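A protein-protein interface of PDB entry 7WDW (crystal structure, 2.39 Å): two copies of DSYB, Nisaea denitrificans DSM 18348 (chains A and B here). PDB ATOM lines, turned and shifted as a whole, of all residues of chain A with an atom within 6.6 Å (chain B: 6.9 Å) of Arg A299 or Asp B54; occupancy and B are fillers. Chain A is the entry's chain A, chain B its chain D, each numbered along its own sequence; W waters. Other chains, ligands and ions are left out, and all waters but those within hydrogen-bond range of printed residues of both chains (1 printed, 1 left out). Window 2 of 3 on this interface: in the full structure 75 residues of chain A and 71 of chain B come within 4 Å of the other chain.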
ATOM      1  N   PHE A 242       7.307  23.049   9.760  1.00  0.00           N
ATOM      2  CA  PHE A 242       6.564  22.847  10.997  1.00  0.00           C
ATOM      3  C   PHE A 242       6.536  21.379  11.434  1.00  0.00           C
ATOM      4  O   PHE A 242       6.706  21.082  12.613  1.00  0.00           O
ATOM      5  CB  PHE A 242       5.154  23.399  10.870  1.00  0.00           C
ATOM      6  CG  PHE A 242       5.067  24.880  11.092  1.00  0.00           C
ATOM      7  CD1 PHE A 242       5.254  25.770  10.043  1.00  0.00           C
ATOM      8  CD2 PHE A 242       4.807  25.390  12.356  1.00  0.00           C
ATOM      9  CE1 PHE A 242       5.181  27.138  10.253  1.00  0.00           C
ATOM     10  CE2 PHE A 242       4.730  26.757  12.569  1.00  0.00           C
ATOM     11  CZ  PHE A 242       4.916  27.630  11.516  1.00  0.00           C
ATOM     12  N   SER A 243       6.345  20.476  10.473  1.00  0.00           N
ATOM     13  CA  SER A 243       6.266  19.033  10.726  1.00  0.00           C
ATOM     14  C   SER A 243       7.491  18.431  11.398  1.00  0.00           C
ATOM     15  O   SER A 243       7.361  17.486  12.171  1.00  0.00           O
ATOM     16  CB  SER A 243       6.034  18.286   9.414  1.00  0.00           C
ATOM     17  OG  SER A 243       4.656  18.093   9.198  1.00  0.00           O
ATOM     18  N   VAL A 245       9.778  20.073  13.245  1.00  0.00           N
ATOM     19  CA  VAL A 245      10.225  21.007  14.266  1.00  0.00           C
ATOM     20  C   VAL A 245       9.359  20.811  15.523  1.00  0.00           C
ATOM     21  O   VAL A 245       8.152  20.537  15.427  1.00  0.00           O
ATOM     22  CB  VAL A 245      10.120  22.483  13.726  1.00  0.00           C
ATOM     23  CG1 VAL A 245       9.724  23.465  14.811  1.00  0.00           C
ATOM     24  CG2 VAL A 245      11.413  22.908  13.027  1.00  0.00           C
ATOM     25  N   ALA A 246       9.972  20.928  16.697  1.00  0.00           N
ATOM     26  CA  ALA A 246       9.230  20.835  17.954  1.00  0.00           C
ATOM     27  C   ALA A 246       8.044  21.794  17.962  1.00  0.00           C
ATOM     28  O   ALA A 246       8.107  22.896  17.407  1.00  0.00           O
ATOM     29  CB  ALA A 246      10.147  21.103  19.148  1.00  0.00           C
ATOM     30  N   GLY A 247       6.963  21.373  18.598  1.00  0.00           N
ATOM     31  CA  GLY A 247       5.749  22.155  18.592  1.00  0.00           C
ATOM     32  C   GLY A 247       5.763  23.427  19.413  1.00  0.00           C
ATOM     33  O   GLY A 247       4.870  24.263  19.290  1.00  0.00           O
ATOM     34  N   ASP A 248       6.759  23.578  20.271  1.00  0.00           N
ATOM     35  CA  ASP A 248       6.853  24.785  21.085  1.00  0.00           C
ATOM     36  C   ASP A 248       7.477  25.951  20.312  1.00  0.00           C
ATOM     37  O   ASP A 248       7.386  27.108  20.723  1.00  0.00           O
ATOM     38  CB  ASP A 248       7.614  24.495  22.378  1.00  0.00           C
ATOM     39  CG  ASP A 248       6.835  23.585  23.313  1.00  0.00           C
ATOM     40  OD1 ASP A 248       5.586  23.599  23.243  1.00  0.00           O
ATOM     41  OD2 ASP A 248       7.468  22.862  24.115  1.00  0.00           O
ATOM     42  N   HIS A 250       6.435  26.673  17.370  1.00  0.00           N
ATOM     43  CA  HIS A 250       5.452  27.054  16.352  1.00  0.00           C
ATOM     44  C   HIS A 250       4.992  28.516  16.396  1.00  0.00           C
ATOM     45  O   HIS A 250       4.858  29.157  15.357  1.00  0.00           O
ATOM     46  CB  HIS A 250       4.256  26.080  16.337  1.00  0.00           C
ATOM     47  CG  HIS A 250       4.543  24.786  15.632  1.00  0.00           C
ATOM     48  ND1 HIS A 250       3.553  23.979  15.115  1.00  0.00           N
ATOM     49  CD2 HIS A 250       5.715  24.172  15.340  1.00  0.00           C
ATOM     50  CE1 HIS A 250       4.103  22.925  14.541  1.00  0.00           C
ATOM     51  NE2 HIS A 250       5.414  23.023  14.657  1.00  0.00           N
ATOM     52  N   ASP A 251       4.753  29.046  17.587  1.00  0.00           N
ATOM     53  CA  ASP A 251       4.297  30.426  17.706  1.00  0.00           C
ATOM     54  C   ASP A 251       5.401  31.394  17.284  1.00  0.00           C
ATOM     55  O   ASP A 251       5.212  32.210  16.386  1.00  0.00           O
ATOM     56  CB  ASP A 251       3.800  30.715  19.126  1.00  0.00           C
ATOM     57  CG  ASP A 251       2.526  29.940  19.468  1.00  0.00           C
ATOM     58  OD1 ASP A 251       1.924  29.351  18.538  1.00  0.00           O
ATOM     59  OD2 ASP A 251       2.116  29.924  20.651  1.00  0.00           O
ATOM     60  N   ARG A 278     -10.582  16.572  12.659  1.00  0.00           N
ATOM     61  CA  ARG A 278      -9.514  15.606  12.913  1.00  0.00           C
ATOM     62  C   ARG A 278      -9.893  14.173  12.569  1.00  0.00           C
ATOM     63  O   ARG A 278      -9.675  13.240  13.352  1.00  0.00           O
ATOM     64  CB  ARG A 278      -8.987  15.729  14.342  1.00  0.00           C
ATOM     65  CG  ARG A 278      -8.029  16.894  14.500  1.00  0.00           C
ATOM     66  CD  ARG A 278      -7.453  17.029  15.896  1.00  0.00           C
ATOM     67  NE  ARG A 278      -6.458  18.097  15.913  1.00  0.00           N
ATOM     68  CZ  ARG A 278      -5.155  17.905  15.747  1.00  0.00           C
ATOM     69  NH1 ARG A 278      -4.669  16.678  15.583  1.00  0.00           N
ATOM     70  NH2 ARG A 278      -4.330  18.940  15.759  1.00  0.00           N
ATOM     71  N   GLN A 288       2.154  13.024   9.554  1.00  0.00           N
ATOM     72  CA  GLN A 288       2.452  13.735  10.802  1.00  0.00           C
ATOM     73  C   GLN A 288       3.080  12.747  11.773  1.00  0.00           C
ATOM     74  O   GLN A 288       4.101  13.029  12.402  1.00  0.00           O
ATOM     75  CB  GLN A 288       1.184  14.328  11.429  1.00  0.00           C
ATOM     76  CG  GLN A 288       0.404  15.262  10.526  1.00  0.00           C
ATOM     77  CD  GLN A 288      -0.527  16.211  11.283  1.00  0.00           C
ATOM     78  OE1 GLN A 288      -1.297  15.800  12.168  1.00  0.00           O
ATOM     79  NE2 GLN A 288      -0.453  17.489  10.939  1.00  0.00           N
ATOM     80  N   THR A 292       6.898  12.414  13.389  1.00  0.00           N
ATOM     81  CA  THR A 292       7.057  12.320  14.834  1.00  0.00           C
ATOM     82  C   THR A 292       8.093  11.260  15.231  1.00  0.00           C
ATOM     83  O   THR A 292       8.689  11.334  16.303  1.00  0.00           O
ATOM     84  CB  THR A 292       5.728  12.030  15.518  1.00  0.00           C
ATOM     85  OG1 THR A 292       4.792  13.079  15.216  1.00  0.00           O
ATOM     86  CG2 THR A 292       5.920  11.923  17.026  1.00  0.00           C
ATOM     87  N   THR A 295      11.143  13.244  15.310  1.00  0.00           N
ATOM     88  CA  THR A 295      10.809  14.577  15.792  1.00  0.00           C
ATOM     89  C   THR A 295       9.833  14.339  16.923  1.00  0.00           C
ATOM     90  O   THR A 295       8.650  14.635  16.802  1.00  0.00           O
ATOM     91  CB  THR A 295      10.049  15.440  14.741  1.00  0.00           C
ATOM     92  OG1 THR A 295      10.766  15.473  13.506  1.00  0.00           O
ATOM     93  CG2 THR A 295       9.868  16.857  15.246  1.00  0.00           C
ATOM     94  N   GLU A 297       9.002  15.735  19.510  1.00  0.00           N
ATOM     95  CA  GLU A 297       8.313  16.881  20.111  1.00  0.00           C
ATOM     96  C   GLU A 297       7.304  17.548  19.172  1.00  0.00           C
ATOM     97  O   GLU A 297       6.657  18.539  19.531  1.00  0.00           O
ATOM     98  CB  GLU A 297       9.322  17.919  20.601  1.00  0.00           C
ATOM     99  CG  GLU A 297      10.113  17.509  21.833  1.00  0.00           C
ATOM    100  CD  GLU A 297      10.062  18.568  22.926  1.00  0.00           C
ATOM    101  OE1 GLU A 297      10.407  19.738  22.646  1.00  0.00           O
ATOM    102  OE2 GLU A 297       9.658  18.234  24.063  1.00  0.00           O
ATOM    103  N   ALA A 298       7.159  16.993  17.974  1.00  0.00           N
ATOM    104  CA  ALA A 298       6.230  17.538  16.992  1.00  0.00           C
ATOM    105  C   ALA A 298       4.815  17.641  17.553  1.00  0.00           C
ATOM    106  O   ALA A 298       4.475  16.988  18.543  1.00  0.00           O
ATOM    107  CB  ALA A 298       6.238  16.689  15.726  1.00  0.00           C
ATOM    108  N   ARG A 299       4.002  18.478  16.923  1.00  0.00           N
ATOM    109  CA  ARG A 299       2.589  18.560  17.246  1.00  0.00           C
ATOM    110  C   ARG A 299       1.767  18.479  15.964  1.00  0.00           C
ATOM    111  O   ARG A 299       2.314  18.490  14.865  1.00  0.00           O
ATOM    112  CB  ARG A 299       2.265  19.832  18.047  1.00  0.00           C
ATOM    113  CG  ARG A 299       2.897  21.123  17.500  1.00  0.00           C
ATOM    114  CD  ARG A 299       2.392  22.368  18.248  1.00  0.00           C
ATOM    115  NE  ARG A 299       0.937  22.514  18.151  1.00  0.00           N
ATOM    116  CZ  ARG A 299       0.309  23.244  17.232  1.00  0.00           C
ATOM    117  NH1 ARG A 299       1.004  23.912  16.312  1.00  0.00           N
ATOM    118  NH2 ARG A 299      -1.019  23.309  17.228  1.00  0.00           N
ATOM    119  N   SER A 300       0.452  18.400  16.109  1.00  0.00           N
ATOM    120  CA  SER A 300      -0.418  18.210  14.959  1.00  0.00           C
ATOM    121  C   SER A 300      -1.035  19.504  14.439  1.00  0.00           C
ATOM    122  O   SER A 300      -1.889  20.096  15.103  1.00  0.00           O
ATOM    123  CB  SER A 300      -1.534  17.237  15.311  1.00  0.00           C
ATOM    124  OG  SER A 300      -2.431  17.122  14.226  1.00  0.00           O
ATOM    125  N   LEU A 301      -0.618  19.921  13.245  1.00  0.00           N
ATOM    126  CA  LEU A 301      -1.196  21.090  12.560  1.00  0.00           C
ATOM    127  C   LEU A 301      -2.577  20.823  11.963  1.00  0.00           C
ATOM    128  O   LEU A 301      -2.700  20.032  11.040  1.00  0.00           O
ATOM    129  CB  LEU A 301      -0.278  21.523  11.411  1.00  0.00           C
ATOM    130  CG  LEU A 301       1.066  22.188  11.718  1.00  0.00           C
ATOM    131  CD1 LEU A 301       1.834  22.477  10.424  1.00  0.00           C
ATOM    132  CD2 LEU A 301       0.857  23.468  12.533  1.00  0.00           C
ATOM    133  N   ASP A 302      -3.615  21.485  12.458  1.00  0.00           N
ATOM    134  CA  ASP A 302      -4.889  21.483  11.734  1.00  0.00           C
ATOM    135  C   ASP A 302      -5.146  22.851  11.096  1.00  0.00           C
ATOM    136  O   ASP A 302      -4.540  23.839  11.482  1.00  0.00           O
ATOM    137  CB  ASP A 302      -6.067  21.034  12.614  1.00  0.00           C
ATOM    138  CG  ASP A 302      -6.287  21.929  13.814  1.00  0.00           C
ATOM    139  OD1 ASP A 302      -5.588  21.743  14.836  1.00  0.00           O
ATOM    140  OD2 ASP A 302      -7.178  22.803  13.743  1.00  0.00           O
ATOM    141  N   TRP A 305      -6.568  25.760  13.675  1.00  0.00           N
ATOM    142  CA  TRP A 305      -5.508  26.309  14.502  1.00  0.00           C
ATOM    143  C   TRP A 305      -4.558  27.186  13.687  1.00  0.00           C
ATOM    144  O   TRP A 305      -4.126  28.245  14.148  1.00  0.00           O
ATOM    145  CB  TRP A 305      -4.710  25.218  15.206  1.00  0.00           C
ATOM    146  CG  TRP A 305      -3.586  25.804  15.991  1.00  0.00           C
ATOM    147  CD1 TRP A 305      -3.600  26.130  17.315  1.00  0.00           C
ATOM    148  CD2 TRP A 305      -2.283  26.180  15.499  1.00  0.00           C
ATOM    149  NE1 TRP A 305      -2.390  26.679  17.681  1.00  0.00           N
ATOM    150  CE2 TRP A 305      -1.565  26.719  16.588  1.00  0.00           C
ATOM    151  CE3 TRP A 305      -1.658  26.110  14.249  1.00  0.00           C
ATOM    152  CZ2 TRP A 305      -0.244  27.182  16.466  1.00  0.00           C
ATOM    153  CZ3 TRP A 305      -0.346  26.578  14.127  1.00  0.00           C
ATOM    154  CH2 TRP A 305       0.343  27.107  15.231  1.00  0.00           C
ATOM    155  N   VAL B  42      -7.994  14.864  24.930  1.00  0.00           N
ATOM    156  CA  VAL B  42      -6.570  14.697  24.711  1.00  0.00           C
ATOM    157  C   VAL B  42      -5.788  14.747  26.018  1.00  0.00           C
ATOM    158  O   VAL B  42      -4.875  13.953  26.228  1.00  0.00           O
ATOM    159  CB  VAL B  42      -6.037  15.735  23.704  1.00  0.00           C
ATOM    160  CG1 VAL B  42      -4.523  15.790  23.747  1.00  0.00           C
ATOM    161  CG2 VAL B  42      -6.543  15.415  22.296  1.00  0.00           C
ATOM    162  N   ALA B  46      -3.860  11.850  27.662  1.00  0.00           N
ATOM    163  CA  ALA B  46      -2.449  12.095  27.947  1.00  0.00           C
ATOM    164  C   ALA B  46      -2.131  11.511  29.317  1.00  0.00           C
ATOM    165  O   ALA B  46      -1.090  10.887  29.523  1.00  0.00           O
ATOM    166  CB  ALA B  46      -2.131  13.583  27.902  1.00  0.00           C
ATOM    167  N   LEU B  51       1.332   9.795  28.045  1.00  0.00           N
ATOM    168  CA  LEU B  51       1.884  10.369  26.819  1.00  0.00           C
ATOM    169  C   LEU B  51       1.647  11.865  26.834  1.00  0.00           C
ATOM    170  O   LEU B  51       0.718  12.337  27.483  1.00  0.00           O
ATOM    171  CB  LEU B  51       1.233   9.755  25.573  1.00  0.00           C
ATOM    172  CG  LEU B  51       1.614   8.319  25.200  1.00  0.00           C
ATOM    173  CD1 LEU B  51       0.741   7.803  24.059  1.00  0.00           C
ATOM    174  CD2 LEU B  51       3.100   8.198  24.845  1.00  0.00           C
ATOM    175  N   HIS B  52       2.489  12.607  26.125  1.00  0.00           N
ATOM    176  CA  HIS B  52       2.302  14.048  26.003  1.00  0.00           C
ATOM    177  C   HIS B  52       0.978  14.315  25.287  1.00  0.00           C
ATOM    178  O   HIS B  52       0.620  13.597  24.351  1.00  0.00           O
ATOM    179  CB  HIS B  52       3.479  14.694  25.253  1.00  0.00           C
ATOM    180  CG  HIS B  52       3.542  16.185  25.400  1.00  0.00           C
ATOM    181  ND1 HIS B  52       2.681  17.035  24.740  1.00  0.00           N
ATOM    182  CD2 HIS B  52       4.353  16.975  26.145  1.00  0.00           C
ATOM    183  CE1 HIS B  52       2.965  18.284  25.065  1.00  0.00           C
ATOM    184  NE2 HIS B  52       3.975  18.274  25.919  1.00  0.00           N
ATOM    185  N   PRO B  53       0.231  15.328  25.744  1.00  0.00           N
ATOM    186  CA  PRO B  53      -1.051  15.652  25.112  1.00  0.00           C
ATOM    187  C   PRO B  53      -0.882  15.914  23.621  1.00  0.00           C
ATOM    188  O   PRO B  53      -1.812  15.723  22.847  1.00  0.00           O
ATOM    189  CB  PRO B  53      -1.480  16.936  25.826  1.00  0.00           C
ATOM    190  CG  PRO B  53      -0.823  16.858  27.148  1.00  0.00           C
ATOM    191  CD  PRO B  53       0.501  16.172  26.915  1.00  0.00           C
ATOM    192  N   ASP B  54       0.299  16.343  23.210  1.00  0.00           N
ATOM    193  CA  ASP B  54       0.491  16.612  21.797  1.00  0.00           C
ATOM    194  C   ASP B  54       0.746  15.348  20.990  1.00  0.00           C
ATOM    195  O   ASP B  54       0.157  15.172  19.923  1.00  0.00           O
ATOM    196  CB  ASP B  54       1.538  17.706  21.572  1.00  0.00           C
ATOM    197  CG  ASP B  54       0.936  19.092  21.746  1.00  0.00           C
ATOM    198  OD1 ASP B  54      -0.299  19.216  21.519  1.00  0.00           O
ATOM    199  OD2 ASP B  54       1.668  20.034  22.119  1.00  0.00           O
ATOM    200  N   ARG B  55       1.588  14.461  21.516  1.00  0.00           N
ATOM    201  CA  ARG B  55       1.789  13.157  20.888  1.00  0.00           C
ATOM    202  C   ARG B  55       0.514  12.300  20.885  1.00  0.00           C
ATOM    203  O   ARG B  55       0.288  11.557  19.934  1.00  0.00           O
ATOM    204  CB  ARG B  55       2.964  12.393  21.509  1.00  0.00           C
ATOM    205  CG  ARG B  55       4.334  12.721  20.919  1.00  0.00           C
ATOM    206  CD  ARG B  55       5.062  13.789  21.744  1.00  0.00           C
ATOM    207  NE  ARG B  55       4.809  15.130  21.240  1.00  0.00           N
ATOM    208  CZ  ARG B  55       5.198  16.252  21.839  1.00  0.00           C
ATOM    209  NH1 ARG B  55       5.860  16.219  22.985  1.00  0.00           N
ATOM    210  NH2 ARG B  55       4.909  17.417  21.285  1.00  0.00           N
ATOM    211  N   VAL B  56      -0.329  12.409  21.916  1.00  0.00           N
ATOM    212  CA  VAL B  56      -1.615  11.692  21.882  1.00  0.00           C
ATOM    213  C   VAL B  56      -2.558  12.241  20.818  1.00  0.00           C
ATOM    214  O   VAL B  56      -3.302  11.490  20.186  1.00  0.00           O
ATOM    215  CB  VAL B  56      -2.363  11.640  23.245  1.00  0.00           C
ATOM    216  CG1 VAL B  56      -1.806  10.534  24.125  1.00  0.00           C
ATOM    217  CG2 VAL B  56      -2.312  12.955  23.942  1.00  0.00           C
ATOM    218  N   GLN B  57      -2.535  13.551  20.632  1.00  0.00           N
ATOM    219  CA  GLN B  57      -3.378  14.175  19.631  1.00  0.00           C
ATOM    220  C   GLN B  57      -2.968  13.696  18.246  1.00  0.00           C
ATOM    221  O   GLN B  57      -3.810  13.300  17.467  1.00  0.00           O
ATOM    222  CB  GLN B  57      -3.301  15.702  19.719  1.00  0.00           C
ATOM    223  CG  GLN B  57      -4.270  16.400  18.797  1.00  0.00           C
ATOM    224  CD  GLN B  57      -4.384  17.886  19.077  1.00  0.00           C
ATOM    225  OE1 GLN B  57      -5.489  18.416  19.188  1.00  0.00           O
ATOM    226  NE2 GLN B  57      -3.242  18.573  19.174  1.00  0.00           N
ATOM    227  N   THR B  58      -1.674  13.735  17.944  1.00  0.00           N
ATOM    228  CA  THR B  58      -1.175  13.222  16.670  1.00  0.00           C
ATOM    229  C   THR B  58      -1.532  11.746  16.485  1.00  0.00           C
ATOM    230  O   THR B  58      -1.887  11.317  15.393  1.00  0.00           O
ATOM    231  CB  THR B  58       0.350  13.344  16.579  1.00  0.00           C
ATOM    232  OG1 THR B  58       0.714  14.727  16.574  1.00  0.00           O
ATOM    233  CG2 THR B  58       0.871  12.675  15.310  1.00  0.00           C
ATOM    234  N   LEU B  59      -1.442  10.979  17.561  1.00  0.00           N
ATOM    235  CA  LEU B  59      -1.675   9.546  17.480  1.00  0.00           C
ATOM    236  C   LEU B  59      -3.145   9.245  17.246  1.00  0.00           C
ATOM    237  O   LEU B  59      -3.494   8.482  16.340  1.00  0.00           O
ATOM    238  CB  LEU B  59      -1.176   8.825  18.745  1.00  0.00           C
ATOM    239  CG  LEU B  59      -1.496   7.323  18.787  1.00  0.00           C
ATOM    240  CD1 LEU B  59      -1.035   6.689  17.486  1.00  0.00           C
ATOM    241  CD2 LEU B  59      -0.866   6.597  19.996  1.00  0.00           C
HETATM  242  O   HOH W   1      -0.590  17.911  18.360  1.00  0.00           O
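ND1 of His A250 is in hydrogen-bond range of NH1 of Arg A299, at 2.8 Å.
OG of Ser A300 sits at hydrogen-bond distance from NH1 of Arg A278 (2.7 Å).
OD1 of Asp A302 lies within salt-bridge range of NH2 of Arg A278 (3.2 Å).
The side-chain hydroxyl (OG1) of Thr A292 sits at hydrogen-bond distance from the backbone carbonyl oxygen (O) of Gln A288 (2.9 Å).
The side-chain hydroxyl (OG) of Ser A300 lies within hydrogen-bond range of the side-chain amide oxygen (OE1) of Gln A288, 2.7 Å away.
The side-chain hydroxyl (OG1) of Thr B58 lies within hydrogen-bond range of the backbone carbonyl oxygen (O) of Asp B54 (3.4 Å).
Printed residues of chain B within 4 Å of Arg A299: Asp B54 (3.9996 Å) and Thr B58 (3.9 Å).
Of the printed residues of chain A, Asp B54 touches Arg A299 (3.9996 Å).
Printed residues of chain B within 4 Å of Thr A292: Thr B58 (3.9 Å).
Of the printed residues of chain B, Glu A297 touches Arg B55.
Of the printed residues of chain A, Thr B58 touches Thr A292, Arg A299 and Ser A300.
Of the printed residues of chain A, Arg B55 touches Glu A297 and Ala A298.
Printed residues of chain B within 4 Å of Ala A298: Arg B55.
Val A245 touches none of the printed residues of chain B.
The nearest printed residue of chain B that does not touch Arg A299 is Arg B55 (4.6 Å).
The nearest printed residue of chain B that does not touch Glu A297 is Asp B54 (5.6 Å).
Thr B58 touches Thr A292.
Asp B54 touches Arg A299 (CG to CB, 3.9996 Å).
Arg A299 touches Thr B58.
Ser A300 touches Thr B58.
NE of Arg A278 lies within hydrogen-bond range of OE1 of Gln B57.
O of Glu A297 lies within hydrogen-bond range of NH2 of Arg B55, 2.7 Å away.
The backbone carbonyl oxygen of Ala A298 sits at hydrogen-bond distance from the guanidinium group of Arg B55.
Water W1 lies within hydrogen-bond range of the backbone NH (N) of Ser A300 (2.5 Å), the side-chain amide nitrogen (NE2) of Gln B57 (2.9 Å) and the backbone carbonyl oxygen (O) of Asp B54 (3.2 Å).
Printed residues of chain B that touch a printed residue of chain A: Asp B54, Arg B55, Gln B57 and Thr B58.
Along chain B the printed residues that touch a printed residue of chain A span positions 54 to 58.
Of the 19 printed residues of chain A, 6 touch a printed residue of chain B.
Among the printed residues, 7 pairs touch across the chains.
No position is printed for both chains.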
